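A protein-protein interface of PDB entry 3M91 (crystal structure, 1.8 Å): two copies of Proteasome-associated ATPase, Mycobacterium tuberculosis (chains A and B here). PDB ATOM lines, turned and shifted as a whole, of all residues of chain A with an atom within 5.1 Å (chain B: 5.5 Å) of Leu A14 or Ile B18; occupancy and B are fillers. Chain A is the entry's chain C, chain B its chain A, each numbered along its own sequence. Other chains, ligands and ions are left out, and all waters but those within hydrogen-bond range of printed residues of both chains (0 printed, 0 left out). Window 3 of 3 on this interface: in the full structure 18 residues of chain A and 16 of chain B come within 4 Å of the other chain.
Leu A14 touches just these residues of chain B: Ile B11, Leu B14 and Ile B18.
Of the printed residues of chain A, Ile B18 touches Leu A14 (3.7 Å), Arg A17 (3.3 Å), Ile A18 (3.5 Å) and Leu A21 (3.8 Å).
Printed residues of chain B within 4 Å of Arg A17: Ile B18 (3.3 Å).
Of the printed residues of chain A, Leu B21 touches Ile A18 (3.8 Å) and Leu A21 (3.8 Å).
Printed residues of chain B within 4 Å of Ile A11: Ile B11 (3.9 Å) and Leu B14 (3.8 Å).
Of the printed residues of chain A, Arg B17 touches Ile A18 (3.3 Å).
Ile B11 touches its own counterpart, Ile A11.
Leu B14 touches its own counterpart, Leu A14.
Arg A17 touches Ile B18, and with the chains exchanged Ile A18 touches Arg B17.
Ile A18 touches Leu B21, and with the chains exchanged Leu A21 touches Ile B18.
Positions printed for both chains: 11, 13, 14, 15, 16, 17, 18 and 21.
Printed residues of chain B that touch a printed residue of chain A: Ile B11, Leu B14, Arg B17, Ile B18 and Leu B21.
Hydrophobic or aromatic side chains of chain B within 4 Å of the printed part of chain A: Ile B11, Leu B14, Ile B18 and Leu B21.
Of the 10 printed residues of chain A, 5 touch a printed residue of chain B.
Among the printed residues, no Asp or Glu carboxylate lies within 4 Å of a Lys or Arg side-chain nitrogen of the other chain.
Ile A11 touches Ile B11.
Leu B14 touches Ile A11 (CD1 to CD1, 3.8 Å).
Leu A14 touches Ile B11.
O of Leu A14 touches CD1 of Ile B18, 3.7 Å away.
Arg A17 touches Ile B18.
O of Leu B14 touches CD1 of Ile A18, at 3.8 Å.
Ile A18 touches Ile B18 (CG1 to CG1, 3.5 Å).
Leu B21 touches Ile A18.
Leu A21 touches Ile B18 (CD1 to O, 3.8 Å).
Leu A21 touches Leu B21 (CB to CB, 3.8 Å).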
ATOM      1  N   ASP A  10     -23.442  30.508 -27.667  1.00  0.00           N
ATOM      2  CA  ASP A  10     -24.654  29.764 -27.370  1.00  0.00           C
ATOM      3  C   ASP A  10     -24.932  28.779 -28.478  1.00  0.00           C
ATOM      4  O   ASP A  10     -25.208  27.599 -28.202  1.00  0.00           O
ATOM      5  CB  ASP A  10     -25.852  30.693 -27.194  1.00  0.00           C
ATOM      6  CG  ASP A  10     -25.760  31.528 -25.936  1.00  0.00           C
ATOM      7  OD1 ASP A  10     -24.885  31.261 -25.081  1.00  0.00           O
ATOM      8  OD2 ASP A  10     -26.573  32.459 -25.804  1.00  0.00           O
ATOM      9  N   ILE A  11     -24.868  29.280 -29.718  1.00  0.00           N
ATOM     10  CA  ILE A  11     -24.975  28.469 -30.927  1.00  0.00           C
ATOM     11  C   ILE A  11     -24.028  27.271 -30.810  1.00  0.00           C
ATOM     12  O   ILE A  11     -24.465  26.123 -30.935  1.00  0.00           O
ATOM     13  CB  ILE A  11     -24.705  29.300 -32.225  1.00  0.00           C
ATOM     14  CG1 ILE A  11     -25.909  30.189 -32.585  1.00  0.00           C
ATOM     15  CG2 ILE A  11     -24.295  28.413 -33.393  1.00  0.00           C
ATOM     16  CD1 ILE A  11     -27.233  29.491 -32.835  1.00  0.00           C
ATOM     17  N   HIS A  12     -22.759  27.544 -30.503  1.00  0.00           N
ATOM     18  CA  HIS A  12     -21.725  26.504 -30.415  1.00  0.00           C
ATOM     19  C   HIS A  12     -22.016  25.440 -29.345  1.00  0.00           C
ATOM     20  O   HIS A  12     -21.676  24.274 -29.535  1.00  0.00           O
ATOM     21  CB  HIS A  12     -20.334  27.133 -30.201  1.00  0.00           C
ATOM     22  CG  HIS A  12     -19.269  26.613 -31.131  1.00  0.00           C
ATOM     23  ND1 HIS A  12     -18.564  25.446 -30.888  1.00  0.00           N
ATOM     24  CD2 HIS A  12     -18.775  27.117 -32.292  1.00  0.00           C
ATOM     25  CE1 HIS A  12     -17.691  25.249 -31.865  1.00  0.00           C
ATOM     26  NE2 HIS A  12     -17.799  26.246 -32.729  1.00  0.00           N
ATOM     27  N   GLN A  13     -22.662  25.841 -28.251  1.00  0.00           N
ATOM     28  CA  GLN A  13     -22.960  24.933 -27.139  1.00  0.00           C
ATOM     29  C   GLN A  13     -24.269  24.158 -27.327  1.00  0.00           C
ATOM     30  O   GLN A  13     -24.430  23.027 -26.846  1.00  0.00           O
ATOM     31  CB  GLN A  13     -22.932  25.677 -25.802  1.00  0.00           C
ATOM     32  CG  GLN A  13     -21.509  26.088 -25.422  1.00  0.00           C
ATOM     33  CD  GLN A  13     -21.358  26.552 -23.977  1.00  0.00           C
ATOM     34  OE1 GLN A  13     -21.061  25.741 -23.087  1.00  0.00           O
ATOM     35  NE2 GLN A  13     -21.524  27.873 -23.740  1.00  0.00           N
ATOM     36  N   LEU A  14     -25.184  24.782 -28.053  1.00  0.00           N
ATOM     37  CA  LEU A  14     -26.367  24.113 -28.525  1.00  0.00           C
ATOM     38  C   LEU A  14     -26.013  23.080 -29.578  1.00  0.00           C
ATOM     39  O   LEU A  14     -26.617  22.000 -29.622  1.00  0.00           O
ATOM     40  CB  LEU A  14     -27.375  25.107 -29.085  1.00  0.00           C
ATOM     41  CG  LEU A  14     -28.189  25.886 -28.054  1.00  0.00           C
ATOM     42  CD1 LEU A  14     -29.416  26.456 -28.749  1.00  0.00           C
ATOM     43  CD2 LEU A  14     -28.587  25.052 -26.825  1.00  0.00           C
ATOM     44  N   GLU A  15     -25.046  23.397 -30.427  1.00  0.00           N
ATOM     45  CA  GLU A  15     -24.658  22.457 -31.447  1.00  0.00           C
ATOM     46  C   GLU A  15     -23.942  21.273 -30.831  1.00  0.00           C
ATOM     47  O   GLU A  15     -24.096  20.140 -31.301  1.00  0.00           O
ATOM     48  CB  GLU A  15     -23.801  23.103 -32.518  1.00  0.00           C
ATOM     49  CG  GLU A  15     -24.608  23.785 -33.608  1.00  0.00           C
ATOM     50  CD  GLU A  15     -23.794  24.863 -34.387  1.00  0.00           C
ATOM     51  OE1 GLU A  15     -22.620  25.159 -34.040  1.00  0.00           O
ATOM     52  OE2 GLU A  15     -24.337  25.401 -35.369  1.00  0.00           O
ATOM     53  N   ALA A  16     -23.175  21.516 -29.772  1.00  0.00           N
ATOM     54  CA  ALA A  16     -22.373  20.445 -29.202  1.00  0.00           C
ATOM     55  C   ALA A  16     -23.232  19.471 -28.360  1.00  0.00           C
ATOM     56  O   ALA A  16     -22.899  18.283 -28.237  1.00  0.00           O
ATOM     57  CB  ALA A  16     -21.198  20.999 -28.407  1.00  0.00           C
ATOM     58  N   ARG A  17     -24.321  19.996 -27.792  1.00  0.00           N
ATOM     59  CA  ARG A  17     -25.319  19.216 -27.085  1.00  0.00           C
ATOM     60  C   ARG A  17     -26.097  18.328 -28.081  1.00  0.00           C
ATOM     61  O   ARG A  17     -26.309  17.128 -27.813  1.00  0.00           O
ATOM     62  CB  ARG A  17     -26.229  20.143 -26.268  1.00  0.00           C
ATOM     63  CG  ARG A  17     -27.648  19.620 -26.022  1.00  0.00           C
ATOM     64  CD  ARG A  17     -27.723  18.371 -25.116  1.00  0.00           C
ATOM     65  NE  ARG A  17     -28.347  18.642 -23.819  1.00  0.00           N
ATOM     66  CZ  ARG A  17     -27.670  19.006 -22.733  1.00  0.00           C
ATOM     67  NH1 ARG A  17     -26.336  19.121 -22.774  1.00  0.00           N
ATOM     68  NH2 ARG A  17     -28.324  19.255 -21.607  1.00  0.00           N
ATOM     69  N   ILE A  18     -26.495  18.899 -29.217  1.00  0.00           N
ATOM     70  CA  ILE A  18     -27.032  18.123 -30.342  1.00  0.00           C
ATOM     71  C   ILE A  18     -26.095  16.997 -30.807  1.00  0.00           C
ATOM     72  O   ILE A  18     -26.548  15.840 -30.889  1.00  0.00           O
ATOM     73  CB  ILE A  18     -27.439  19.010 -31.553  1.00  0.00           C
ATOM     74  CG1 ILE A  18     -28.831  19.626 -31.320  1.00  0.00           C
ATOM     75  CG2 ILE A  18     -27.371  18.232 -32.898  1.00  0.00           C
ATOM     76  CD1 ILE A  18     -29.144  20.835 -32.207  1.00  0.00           C
ATOM     77  N   LEU A  21     -26.246  14.255 -28.035  1.00  0.00           N
ATOM     78  CA  LEU A  21     -27.448  13.460 -28.070  1.00  0.00           C
ATOM     79  C   LEU A  21     -27.489  12.573 -29.310  1.00  0.00           C
ATOM     80  O   LEU A  21     -27.897  11.406 -29.215  1.00  0.00           O
ATOM     81  CB  LEU A  21     -28.693  14.333 -28.014  1.00  0.00           C
ATOM     82  CG  LEU A  21     -28.930  15.069 -26.704  1.00  0.00           C
ATOM     83  CD1 LEU A  21     -30.029  16.104 -26.952  1.00  0.00           C
ATOM     84  CD2 LEU A  21     -29.349  14.160 -25.603  1.00  0.00           C
ATOM     85  N   ILE B  11     -31.811  29.834 -32.534  1.00  0.00           N
ATOM     86  CA  ILE B  11     -31.861  29.407 -31.139  1.00  0.00           C
ATOM     87  C   ILE B  11     -33.090  28.525 -30.871  1.00  0.00           C
ATOM     88  O   ILE B  11     -32.958  27.482 -30.233  1.00  0.00           O
ATOM     89  CB  ILE B  11     -31.807  30.613 -30.150  1.00  0.00           C
ATOM     90  CG1 ILE B  11     -30.387  31.207 -30.059  1.00  0.00           C
ATOM     91  CG2 ILE B  11     -32.363  30.253 -28.782  1.00  0.00           C
ATOM     92  CD1 ILE B  11     -29.282  30.283 -29.609  1.00  0.00           C
ATOM     93  N   GLN B  13     -34.894  26.775 -33.129  1.00  0.00           N
ATOM     94  CA  GLN B  13     -34.810  25.552 -33.946  1.00  0.00           C
ATOM     95  C   GLN B  13     -33.809  24.531 -33.409  1.00  0.00           C
ATOM     96  O   GLN B  13     -34.020  23.312 -33.506  1.00  0.00           O
ATOM     97  CB  GLN B  13     -34.493  25.880 -35.406  1.00  0.00           C
ATOM     98  CG  GLN B  13     -35.650  26.564 -36.121  1.00  0.00           C
ATOM     99  CD  GLN B  13     -35.402  26.758 -37.611  1.00  0.00           C
ATOM    100  OE1 GLN B  13     -35.704  25.867 -38.409  1.00  0.00           O
ATOM    101  NE2 GLN B  13     -34.875  27.933 -37.996  1.00  0.00           N
ATOM    102  N   LEU B  14     -32.727  25.049 -32.844  1.00  0.00           N
ATOM    103  CA  LEU B  14     -31.762  24.227 -32.177  1.00  0.00           C
ATOM    104  C   LEU B  14     -32.317  23.716 -30.877  1.00  0.00           C
ATOM    105  O   LEU B  14     -32.014  22.595 -30.490  1.00  0.00           O
ATOM    106  CB  LEU B  14     -30.457  24.956 -31.923  1.00  0.00           C
ATOM    107  CG  LEU B  14     -29.628  25.315 -33.153  1.00  0.00           C
ATOM    108  CD1 LEU B  14     -28.245  25.799 -32.692  1.00  0.00           C
ATOM    109  CD2 LEU B  14     -29.531  24.193 -34.202  1.00  0.00           C
ATOM    110  N   GLU B  15     -33.130  24.520 -30.207  1.00  0.00           N
ATOM    111  CA  GLU B  15     -33.758  24.044 -28.987  1.00  0.00           C
ATOM    112  C   GLU B  15     -34.764  22.934 -29.271  1.00  0.00           C
ATOM    113  O   GLU B  15     -34.901  22.002 -28.470  1.00  0.00           O
ATOM    114  CB  GLU B  15     -34.414  25.171 -28.202  1.00  0.00           C
ATOM    115  CG  GLU B  15     -33.450  25.916 -27.264  1.00  0.00           C
ATOM    116  CD  GLU B  15     -33.991  27.294 -26.798  1.00  0.00           C
ATOM    117  OE1 GLU B  15     -34.917  27.864 -27.437  1.00  0.00           O
ATOM    118  OE2 GLU B  15     -33.493  27.793 -25.769  1.00  0.00           O
ATOM    119  N   ALA B  16     -35.453  23.021 -30.408  1.00  0.00           N
ATOM    120  CA  ALA B  16     -36.502  22.057 -30.748  1.00  0.00           C
ATOM    121  C   ALA B  16     -35.942  20.710 -31.269  1.00  0.00           C
ATOM    122  O   ALA B  16     -36.595  19.661 -31.146  1.00  0.00           O
ATOM    123  CB  ALA B  16     -37.484  22.661 -31.749  1.00  0.00           C
ATOM    124  N   ARG B  17     -34.750  20.767 -31.869  1.00  0.00           N
ATOM    125  CA  ARG B  17     -34.009  19.595 -32.283  1.00  0.00           C
ATOM    126  C   ARG B  17     -33.469  18.850 -31.042  1.00  0.00           C
ATOM    127  O   ARG B  17     -33.646  17.622 -30.930  1.00  0.00           O
ATOM    128  CB  ARG B  17     -32.900  19.984 -33.261  1.00  0.00           C
ATOM    129  CG  ARG B  17     -31.733  19.019 -33.280  1.00  0.00           C
ATOM    130  CD  ARG B  17     -32.130  17.664 -33.869  1.00  0.00           C
ATOM    131  NE  ARG B  17     -31.551  17.463 -35.192  1.00  0.00           N
ATOM    132  CZ  ARG B  17     -32.195  17.713 -36.321  1.00  0.00           C
ATOM    133  NH1 ARG B  17     -33.454  18.155 -36.279  1.00  0.00           N
ATOM    134  NH2 ARG B  17     -31.586  17.520 -37.490  1.00  0.00           N
ATOM    135  N   ILE B  18     -32.825  19.576 -30.134  1.00  0.00           N
ATOM    136  CA  ILE B  18     -32.487  19.072 -28.811  1.00  0.00           C
ATOM    137  C   ILE B  18     -33.675  18.429 -28.104  1.00  0.00           C
ATOM    138  O   ILE B  18     -33.543  17.264 -27.685  1.00  0.00           O
ATOM    139  CB  ILE B  18     -31.856  20.139 -27.894  1.00  0.00           C
ATOM    140  CG1 ILE B  18     -30.354  20.272 -28.191  1.00  0.00           C
ATOM    141  CG2 ILE B  18     -32.124  19.854 -26.389  1.00  0.00           C
ATOM    142  CD1 ILE B  18     -29.737  21.584 -27.686  1.00  0.00           C
ATOM    143  N   ASP B  19     -34.812  19.131 -27.976  1.00  0.00           N
ATOM    144  CA  ASP B  19     -36.017  18.522 -27.384  1.00  0.00           C
ATOM    145  C   ASP B  19     -36.403  17.185 -28.034  1.00  0.00           C
ATOM    146  O   ASP B  19     -36.754  16.223 -27.322  1.00  0.00           O
ATOM    147  CB  ASP B  19     -37.208  19.441 -27.467  1.00  0.00           C
ATOM    148  CG  ASP B  19     -37.068  20.651 -26.547  1.00  0.00           C
ATOM    149  OD1 ASP B  19     -36.061  20.727 -25.797  1.00  0.00           O
ATOM    150  OD2 ASP B  19     -37.966  21.532 -26.568  1.00  0.00           O
ATOM    151  N   SER B  20     -36.324  17.173 -29.373  1.00  0.00           N
ATOM    152  CA  SER B  20     -36.630  16.027 -30.211  1.00  0.00           C
ATOM    153  C   SER B  20     -35.705  14.839 -29.919  1.00  0.00           C
ATOM    154  O   SER B  20     -36.195  13.722 -29.685  1.00  0.00           O
ATOM    155  CB  SER B  20     -36.559  16.393 -31.707  1.00  0.00           C
ATOM    156  OG  SER B  20     -36.489  15.212 -32.526  1.00  0.00           O
ATOM    157  N   LEU B  21     -34.394  15.086 -29.955  1.00  0.00           N
ATOM    158  CA  LEU B  21     -33.401  14.081 -29.669  1.00  0.00           C
ATOM    159  C   LEU B  21     -33.507  13.593 -28.233  1.00  0.00           C
ATOM    160  O   LEU B  21     -33.364  12.368 -27.989  1.00  0.00           O
ATOM    161  CB  LEU B  21     -31.975  14.511 -29.976  1.00  0.00           C
ATOM    162  CG  LEU B  21     -31.578  14.808 -31.409  1.00  0.00           C
ATOM    163  CD1 LEU B  21     -30.273  15.585 -31.335  1.00  0.00           C
ATOM    164  CD2 LEU B  21     -31.401  13.607 -32.272  1.00  0.00           C
ATOM    165  N   ALA B  22     -33.823  14.494 -27.317  1.00  0.00           N
ATOM    166  CA  ALA B  22     -34.007  14.133 -25.922  1.00  0.00           C
ATOM    167  C   ALA B  22     -35.175  13.149 -25.728  1.00  0.00           C
ATOM    168  O   ALA B  22     -35.052  12.196 -24.945  1.00  0.00           O
ATOM    169  CB  ALA B  22     -34.193  15.360 -25.058  1.00  0.00           C
ATOM    170  N   ALA B  23     -36.285  13.389 -26.429  1.00  0.00           N
ATOM    171  CA  ALA B  23     -37.462  12.494 -26.408  1.00  0.00           C
ATOM    172  C   ALA B  23     -37.176  11.101 -27.044  1.00  0.00           C
ATOM    173  O   ALA B  23     -37.588  10.086 -26.493  1.00  0.00           O
ATOM    174  CB  ALA B  23     -38.670  13.148 -27.088  1.00  0.00           C
